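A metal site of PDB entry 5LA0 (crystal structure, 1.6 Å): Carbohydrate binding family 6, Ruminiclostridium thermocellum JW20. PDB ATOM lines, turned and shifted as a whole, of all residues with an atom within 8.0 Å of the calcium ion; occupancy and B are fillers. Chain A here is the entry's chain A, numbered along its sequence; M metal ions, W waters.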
ATOM      1  N   ARG A 342      17.130   4.356  17.942  1.00  0.00           N
ATOM      2  CA  ARG A 342      16.677   5.579  18.585  1.00  0.00           C
ATOM      3  C   ARG A 342      16.496   6.715  17.569  1.00  0.00           C
ATOM      4  O   ARG A 342      17.433   7.042  16.807  1.00  0.00           O
ATOM      5  CB  ARG A 342      17.656   6.007  19.670  1.00  0.00           C
ATOM      6  CG  ARG A 342      17.211   7.248  20.476  1.00  0.00           C
ATOM      7  CD  ARG A 342      18.081   7.516  21.675  1.00  0.00           C
ATOM      8  NE  ARG A 342      18.057   6.425  22.657  1.00  0.00           N
ATOM      9  CZ  ARG A 342      18.765   6.422  23.797  1.00  0.00           C
ATOM     10  NH1 ARG A 342      19.572   7.442  24.086  1.00  0.00           N
ATOM     11  NH2 ARG A 342      18.712   5.376  24.604  1.00  0.00           N
ATOM     12  N   ILE A 343      15.307   7.285  17.588  1.00  0.00           N
ATOM     13  CA  ILE A 343      14.965   8.480  16.838  1.00  0.00           C
ATOM     14  C   ILE A 343      14.738   9.631  17.846  1.00  0.00           C
ATOM     15  O   ILE A 343      13.851   9.555  18.680  1.00  0.00           O
ATOM     16  CB  ILE A 343      13.665   8.274  16.026  1.00  0.00           C
ATOM     17  CG1 ILE A 343      13.769   6.976  15.186  1.00  0.00           C
ATOM     18  CG2 ILE A 343      13.343   9.480  15.139  1.00  0.00           C
ATOM     19  CD1 ILE A 343      12.470   6.585  14.543  1.00  0.00           C
ATOM     20  N   GLU A 344      15.553  10.680  17.766  1.00  0.00           N
ATOM     21  CA  GLU A 344      15.465  11.776  18.688  1.00  0.00           C
ATOM     22  C   GLU A 344      14.159  12.517  18.387  1.00  0.00           C
ATOM     23  O   GLU A 344      13.798  12.751  17.212  1.00  0.00           O
ATOM     24  CB  GLU A 344      16.698  12.702  18.609  1.00  0.00           C
ATOM     25  CG  GLU A 344      17.999  12.062  19.084  1.00  0.00           C
ATOM     26  CD  GLU A 344      17.971  11.634  20.553  1.00  0.00           C
ATOM     27  OE1 GLU A 344      17.133  12.170  21.335  1.00  0.00           O
ATOM     28  OE2 GLU A 344      18.785  10.753  20.908  1.00  0.00           O
ATOM     29  N   ALA A 345      13.444  12.875  19.435  1.00  0.00           N
ATOM     30  CA  ALA A 345      12.123  13.539  19.286  1.00  0.00           C
ATOM     31  C   ALA A 345      12.240  14.863  18.528  1.00  0.00           C
ATOM     32  O   ALA A 345      11.369  15.225  17.732  1.00  0.00           O
ATOM     33  CB  ALA A 345      11.500  13.745  20.650  1.00  0.00           C
ATOM     34  N   GLU A 346      13.350  15.557  18.796  1.00  0.00           N
ATOM     35  CA  GLU A 346      13.722  16.819  18.163  1.00  0.00           C
ATOM     36  C   GLU A 346      14.114  16.718  16.652  1.00  0.00           C
ATOM     37  O   GLU A 346      14.364  17.747  16.006  1.00  0.00           O
ATOM     38  CB  GLU A 346      14.850  17.539  18.974  1.00  0.00           C
ATOM     39  CG  GLU A 346      16.206  16.811  19.100  1.00  0.00           C
ATOM     40  CD  GLU A 346      16.297  15.850  20.294  1.00  0.00           C
ATOM     41  OE1 GLU A 346      15.254  15.267  20.709  1.00  0.00           O
ATOM     42  OE2 GLU A 346      17.387  15.620  20.808  1.00  0.00           O
ATOM     43  N   ASP A 347      14.212  15.484  16.128  1.00  0.00           N
ATOM     44  CA  ASP A 347      14.527  15.213  14.732  1.00  0.00           C
ATOM     45  C   ASP A 347      13.295  14.833  13.891  1.00  0.00           C
ATOM     46  O   ASP A 347      13.390  14.074  12.934  1.00  0.00           O
ATOM     47  CB  ASP A 347      15.580  14.098  14.687  1.00  0.00           C
ATOM     48  CG  ASP A 347      16.970  14.567  15.091  1.00  0.00           C
ATOM     49  OD1 ASP A 347      17.211  15.779  15.211  1.00  0.00           O
ATOM     50  OD2 ASP A 347      17.838  13.696  15.250  1.00  0.00           O
ATOM     51  N   TYR A 369      18.069  24.134  19.356  1.00  0.00           N
ATOM     52  CA  TYR A 369      18.244  23.102  18.308  1.00  0.00           C
ATOM     53  C   TYR A 369      17.684  23.486  16.932  1.00  0.00           C
ATOM     54  O   TYR A 369      18.415  23.464  15.929  1.00  0.00           O
ATOM     55  CB  TYR A 369      17.651  21.776  18.768  1.00  0.00           C
ATOM     56  CG  TYR A 369      18.052  20.578  17.965  1.00  0.00           C
ATOM     57  CD1 TYR A 369      19.373  20.135  17.948  1.00  0.00           C
ATOM     58  CD2 TYR A 369      17.112  19.865  17.217  1.00  0.00           C
ATOM     59  CE1 TYR A 369      19.751  19.035  17.260  1.00  0.00           C
ATOM     60  CE2 TYR A 369      17.491  18.761  16.498  1.00  0.00           C
ATOM     61  CZ  TYR A 369      18.816  18.343  16.523  1.00  0.00           C
ATOM     62  OH  TYR A 369      19.232  17.228  15.827  1.00  0.00           O
ATOM     63  N   ILE A 377      11.535  23.139  21.908  1.00  0.00           N
ATOM     64  CA  ILE A 377      12.659  22.268  22.207  1.00  0.00           C
ATOM     65  C   ILE A 377      13.575  22.945  23.234  1.00  0.00           C
ATOM     66  O   ILE A 377      13.956  24.100  23.094  1.00  0.00           O
ATOM     67  CB  ILE A 377      13.499  21.941  20.939  1.00  0.00           C
ATOM     68  CG1 ILE A 377      12.586  21.475  19.785  1.00  0.00           C
ATOM     69  CG2 ILE A 377      14.619  20.940  21.248  1.00  0.00           C
ATOM     70  CD1 ILE A 377      13.246  21.406  18.465  1.00  0.00           C
ATOM     71  N   GLU A 378      13.939  22.183  24.252  1.00  0.00           N
ATOM     72  CA  GLU A 378      14.850  22.619  25.301  1.00  0.00           C
ATOM     73  C   GLU A 378      15.963  21.565  25.495  1.00  0.00           C
ATOM     74  O   GLU A 378      15.813  20.416  25.083  1.00  0.00           O
ATOM     75  CB  GLU A 378      14.109  22.805  26.608  1.00  0.00           C
ATOM     76  CG  GLU A 378      13.400  21.535  27.057  1.00  0.00           C
ATOM     77  CD  GLU A 378      12.590  21.657  28.332  1.00  0.00           C
ATOM     78  OE1 GLU A 378      12.881  22.504  29.171  1.00  0.00           O
ATOM     79  OE2 GLU A 378      11.647  20.851  28.501  1.00  0.00           O
ATOM     80  N   THR A 380      17.899  18.762  27.561  1.00  0.00           N
ATOM     81  CA  THR A 380      17.479  17.741  28.532  1.00  0.00           C
ATOM     82  C   THR A 380      18.644  17.375  29.439  1.00  0.00           C
ATOM     83  O   THR A 380      19.795  17.379  29.014  1.00  0.00           O
ATOM     84  CB  THR A 380      16.872  16.483  27.902  1.00  0.00           C
ATOM     85  OG1 THR A 380      16.374  15.631  28.925  1.00  0.00           O
ATOM     86  CG2 THR A 380      17.849  15.662  27.087  1.00  0.00           C
ATOM     87  N   ASP A 382      18.382  14.325  30.854  1.00  0.00           N
ATOM     88  CA  ASP A 382      18.311  12.864  30.809  1.00  0.00           C
ATOM     89  C   ASP A 382      19.640  12.273  30.347  1.00  0.00           C
ATOM     90  O   ASP A 382      20.498  12.963  29.766  1.00  0.00           O
ATOM     91  CB  ASP A 382      17.233  12.426  29.806  1.00  0.00           C
ATOM     92  CG  ASP A 382      16.746  10.992  29.977  1.00  0.00           C
ATOM     93  OD1 ASP A 382      16.946  10.337  31.039  1.00  0.00           O
ATOM     94  OD2 ASP A 382      16.115  10.498  28.996  1.00  0.00           O
ATOM     95  N   THR A 383      19.824  10.999  30.642  1.00  0.00           N
ATOM     96  CA  THR A 383      20.960  10.226  30.187  1.00  0.00           C
ATOM     97  C   THR A 383      21.178  10.447  28.710  1.00  0.00           C
ATOM     98  O   THR A 383      20.232  10.312  27.939  1.00  0.00           O
ATOM     99  CB  THR A 383      20.675   8.749  30.372  1.00  0.00           C
ATOM    100  OG1 THR A 383      20.223   8.574  31.709  1.00  0.00           O
ATOM    101  CG2 THR A 383      21.923   7.912  30.123  1.00  0.00           C
ATOM    102  N   GLY A 384      22.397  10.810  28.321  1.00  0.00           N
ATOM    103  CA  GLY A 384      22.750  11.063  26.930  1.00  0.00           C
ATOM    104  C   GLY A 384      22.674  12.524  26.534  1.00  0.00           C
ATOM    105  O   GLY A 384      23.145  12.901  25.467  1.00  0.00           O
ATOM    106  N   GLY A 385      22.066  13.378  27.354  1.00  0.00           N
ATOM    107  CA  GLY A 385      21.982  14.788  27.018  1.00  0.00           C
ATOM    108  C   GLY A 385      21.195  15.069  25.734  1.00  0.00           C
ATOM    109  O   GLY A 385      20.249  14.351  25.387  1.00  0.00           O
ATOM    110  N   GLY A 386      21.606  16.127  25.044  1.00  0.00           N
ATOM    111  CA  GLY A 386      20.889  16.626  23.897  1.00  0.00           C
ATOM    112  C   GLY A 386      19.649  17.372  24.322  1.00  0.00           C
ATOM    113  O   GLY A 386      19.682  18.222  25.227  1.00  0.00           O
ATOM    114  N   TYR A 387      18.522  17.057  23.689  1.00  0.00           N
ATOM    115  CA  TYR A 387      17.336  17.924  23.763  1.00  0.00           C
ATOM    116  C   TYR A 387      16.078  17.112  24.000  1.00  0.00           C
ATOM    117  O   TYR A 387      16.037  15.899  23.784  1.00  0.00           O
ATOM    118  CB  TYR A 387      17.206  18.759  22.485  1.00  0.00           C
ATOM    119  CG  TYR A 387      18.441  19.546  22.189  1.00  0.00           C
ATOM    120  CD1 TYR A 387      18.640  20.820  22.765  1.00  0.00           C
ATOM    121  CD2 TYR A 387      19.457  19.018  21.389  1.00  0.00           C
ATOM    122  CE1 TYR A 387      19.800  21.553  22.522  1.00  0.00           C
ATOM    123  CE2 TYR A 387      20.641  19.747  21.151  1.00  0.00           C
ATOM    124  CZ  TYR A 387      20.791  21.006  21.727  1.00  0.00           C
ATOM    125  OH  TYR A 387      21.910  21.771  21.526  1.00  0.00           O
ATOM    126  N   ASN A 388      15.029  17.785  24.438  1.00  0.00           N
ATOM    127  CA  ASN A 388      13.717  17.156  24.456  1.00  0.00           C
ATOM    128  C   ASN A 388      12.692  18.122  23.898  1.00  0.00           C
ATOM    129  O   ASN A 388      12.838  19.360  23.969  1.00  0.00           O
ATOM    130  CB  ASN A 388      13.349  16.655  25.850  1.00  0.00           C
ATOM    131  CG  ASN A 388      13.152  17.786  26.881  1.00  0.00           C
ATOM    132  OD1 ASN A 388      14.065  18.114  27.623  1.00  0.00           O
ATOM    133  ND2 ASN A 388      11.938  18.341  26.945  1.00  0.00           N
ATOM    134  N   VAL A 389      11.646  17.571  23.350  1.00  0.00           N
ATOM    135  CA  VAL A 389      10.489  18.337  22.978  1.00  0.00           C
ATOM    136  C   VAL A 389       9.687  18.576  24.251  1.00  0.00           C
ATOM    137  O   VAL A 389       9.472  17.656  25.053  1.00  0.00           O
ATOM    138  CB  VAL A 389       9.612  17.629  21.899  1.00  0.00           C
ATOM    139  CG1 VAL A 389       8.305  18.413  21.664  1.00  0.00           C
ATOM    140  CG2 VAL A 389      10.414  17.427  20.619  1.00  0.00           C
ATOM    141  N   ARG A 415      10.564   7.827  25.433  1.00  0.00           N
ATOM    142  CA  ARG A 415      11.269   8.318  26.594  1.00  0.00           C
ATOM    143  C   ARG A 415      10.605   9.627  27.032  1.00  0.00           C
ATOM    144  O   ARG A 415      10.731  10.668  26.363  1.00  0.00           O
ATOM    145  CB  ARG A 415      12.758   8.533  26.287  1.00  0.00           C
ATOM    146  CG  ARG A 415      13.664   8.906  27.435  1.00  0.00           C
ATOM    147  CD  ARG A 415      13.733   7.841  28.502  1.00  0.00           C
ATOM    148  NE  ARG A 415      14.744   8.141  29.488  1.00  0.00           N
ATOM    149  CZ  ARG A 415      15.001   7.372  30.549  1.00  0.00           C
ATOM    150  NH1 ARG A 415      14.332   6.228  30.763  1.00  0.00           N
ATOM    151  NH2 ARG A 415      15.934   7.754  31.404  1.00  0.00           N
ATOM    152  N   TRP A 448      12.726  11.126  34.068  1.00  0.00           N
ATOM    153  CA  TRP A 448      12.518  10.389  32.830  1.00  0.00           C
ATOM    154  C   TRP A 448      12.225   8.920  33.059  1.00  0.00           C
ATOM    155  O   TRP A 448      12.774   8.291  33.986  1.00  0.00           O
ATOM    156  CB  TRP A 448      13.732  10.559  31.923  1.00  0.00           C
ATOM    157  CG  TRP A 448      13.880  11.957  31.494  1.00  0.00           C
ATOM    158  CD1 TRP A 448      14.663  12.901  32.028  1.00  0.00           C
ATOM    159  CD2 TRP A 448      13.173  12.588  30.406  1.00  0.00           C
ATOM    160  NE1 TRP A 448      14.511  14.101  31.360  1.00  0.00           N
ATOM    161  CE2 TRP A 448      13.596  13.928  30.344  1.00  0.00           C
ATOM    162  CE3 TRP A 448      12.222  12.140  29.477  1.00  0.00           C
ATOM    163  CZ2 TRP A 448      13.100  14.825  29.407  1.00  0.00           C
ATOM    164  CZ3 TRP A 448      11.743  13.048  28.528  1.00  0.00           C
ATOM    165  CH2 TRP A 448      12.193  14.347  28.487  1.00  0.00           C
ATOM    166  N   LEU A 475       9.004  14.784  25.717  1.00  0.00           N
ATOM    167  CA  LEU A 475       9.487  13.640  24.931  1.00  0.00           C
ATOM    168  C   LEU A 475      10.932  13.817  24.518  1.00  0.00           C
ATOM    169  O   LEU A 475      11.282  14.785  23.844  1.00  0.00           O
ATOM    170  CB  LEU A 475       8.615  13.470  23.699  1.00  0.00           C
ATOM    171  CG  LEU A 475       8.841  12.254  22.810  1.00  0.00           C
ATOM    172  CD1 LEU A 475       8.506  10.907  23.479  1.00  0.00           C
ATOM    173  CD2 LEU A 475       8.050  12.415  21.506  1.00  0.00           C
ATOM    174  N   ASN A 476      11.771  12.858  24.891  1.00  0.00           N
ATOM    175  CA  ASN A 476      13.213  12.922  24.583  1.00  0.00           C
ATOM    176  C   ASN A 476      13.506  12.180  23.245  1.00  0.00           C
ATOM    177  O   ASN A 476      14.179  12.710  22.373  1.00  0.00           O
ATOM    178  CB  ASN A 476      14.032  12.289  25.717  1.00  0.00           C
ATOM    179  CG  ASN A 476      15.543  12.461  25.556  1.00  0.00           C
ATOM    180  OD1 ASN A 476      16.034  13.089  24.588  1.00  0.00           O
ATOM    181  ND2 ASN A 476      16.278  11.911  26.490  1.00  0.00           N
ATOM    182  N   TRP A 477      12.980  10.961  23.125  1.00  0.00           N
ATOM    183  CA  TRP A 477      13.295  10.119  21.990  1.00  0.00           C
ATOM    184  C   TRP A 477      12.274   8.994  21.893  1.00  0.00           C
ATOM    185  O   TRP A 477      11.483   8.795  22.798  1.00  0.00           O
ATOM    186  CB  TRP A 477      14.762   9.587  22.006  1.00  0.00           C
ATOM    187  CG  TRP A 477      15.274   8.922  23.256  1.00  0.00           C
ATOM    188  CD1 TRP A 477      16.234   9.419  24.094  1.00  0.00           C
ATOM    189  CD2 TRP A 477      14.881   7.645  23.810  1.00  0.00           C
ATOM    190  NE1 TRP A 477      16.459   8.561  25.134  1.00  0.00           N
ATOM    191  CE2 TRP A 477      15.659   7.448  24.980  1.00  0.00           C
ATOM    192  CE3 TRP A 477      13.975   6.650  23.421  1.00  0.00           C
ATOM    193  CZ2 TRP A 477      15.550   6.304  25.750  1.00  0.00           C
ATOM    194  CZ3 TRP A 477      13.865   5.496  24.212  1.00  0.00           C
ATOM    195  CH2 TRP A 477      14.646   5.345  25.364  1.00  0.00           C
ATOM    196  N   ILE A 478      12.337   8.317  20.744  1.00  0.00           N
ATOM    197  CA  ILE A 478      11.510   7.182  20.368  1.00  0.00           C
ATOM    198  C   ILE A 478      12.491   6.051  20.060  1.00  0.00           C
ATOM    199  O   ILE A 478      13.542   6.326  19.525  1.00  0.00           O
ATOM    200  CB  ILE A 478      10.713   7.546  19.103  1.00  0.00           C
ATOM    201  CG1 ILE A 478       9.822   8.742  19.336  1.00  0.00           C
ATOM    202  CG2 ILE A 478       9.853   6.346  18.687  1.00  0.00           C
ATOM    203  CD1 ILE A 478       9.673   9.659  18.140  1.00  0.00           C
HETATM  204 CA    CA M   1      16.411  13.963  22.484  1.00  0.00          CA
HETATM  205  O   HOH W   1      18.700  14.083  23.115  1.00  0.00           O
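O of Asn 476 sits close to N of Ala 345, at 3.0 Å. ND2 of Asn 476 lies within hydrogen-bond range of OD2 of Asp 382, 2.9 Å away. The backbone NH (N) of Asn 476 is in hydrogen-bond range of the backbone carbonyl oxygen (O) of Arg 415, 2.8 Å away.
Of the 24 residues printed, 4 come within 4 Å of the calcium ion. The nearest printed residue that does not touch the calcium ion is Ala 345 (4.4 Å).
The calcium ion is bound by the side-chain carboxylate (OE1) of Glu 344 (2.2 Å), the side-chain amide oxygen (OD1) of Asn 476 (2.3 Å), the backbone carbonyl oxygen (O) of Tyr 387 (2.4 Å), water W1 (2.4 Å), the side-chain carboxylate (OE1) of Glu 346 (2.5 Å), the side-chain carboxylate (OE2) of Glu 346 (2.6 Å) and the backbone carbonyl oxygen (O) of Asn 476 (2.6 Å). The calcium ion has seven donor atoms within binding distance.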
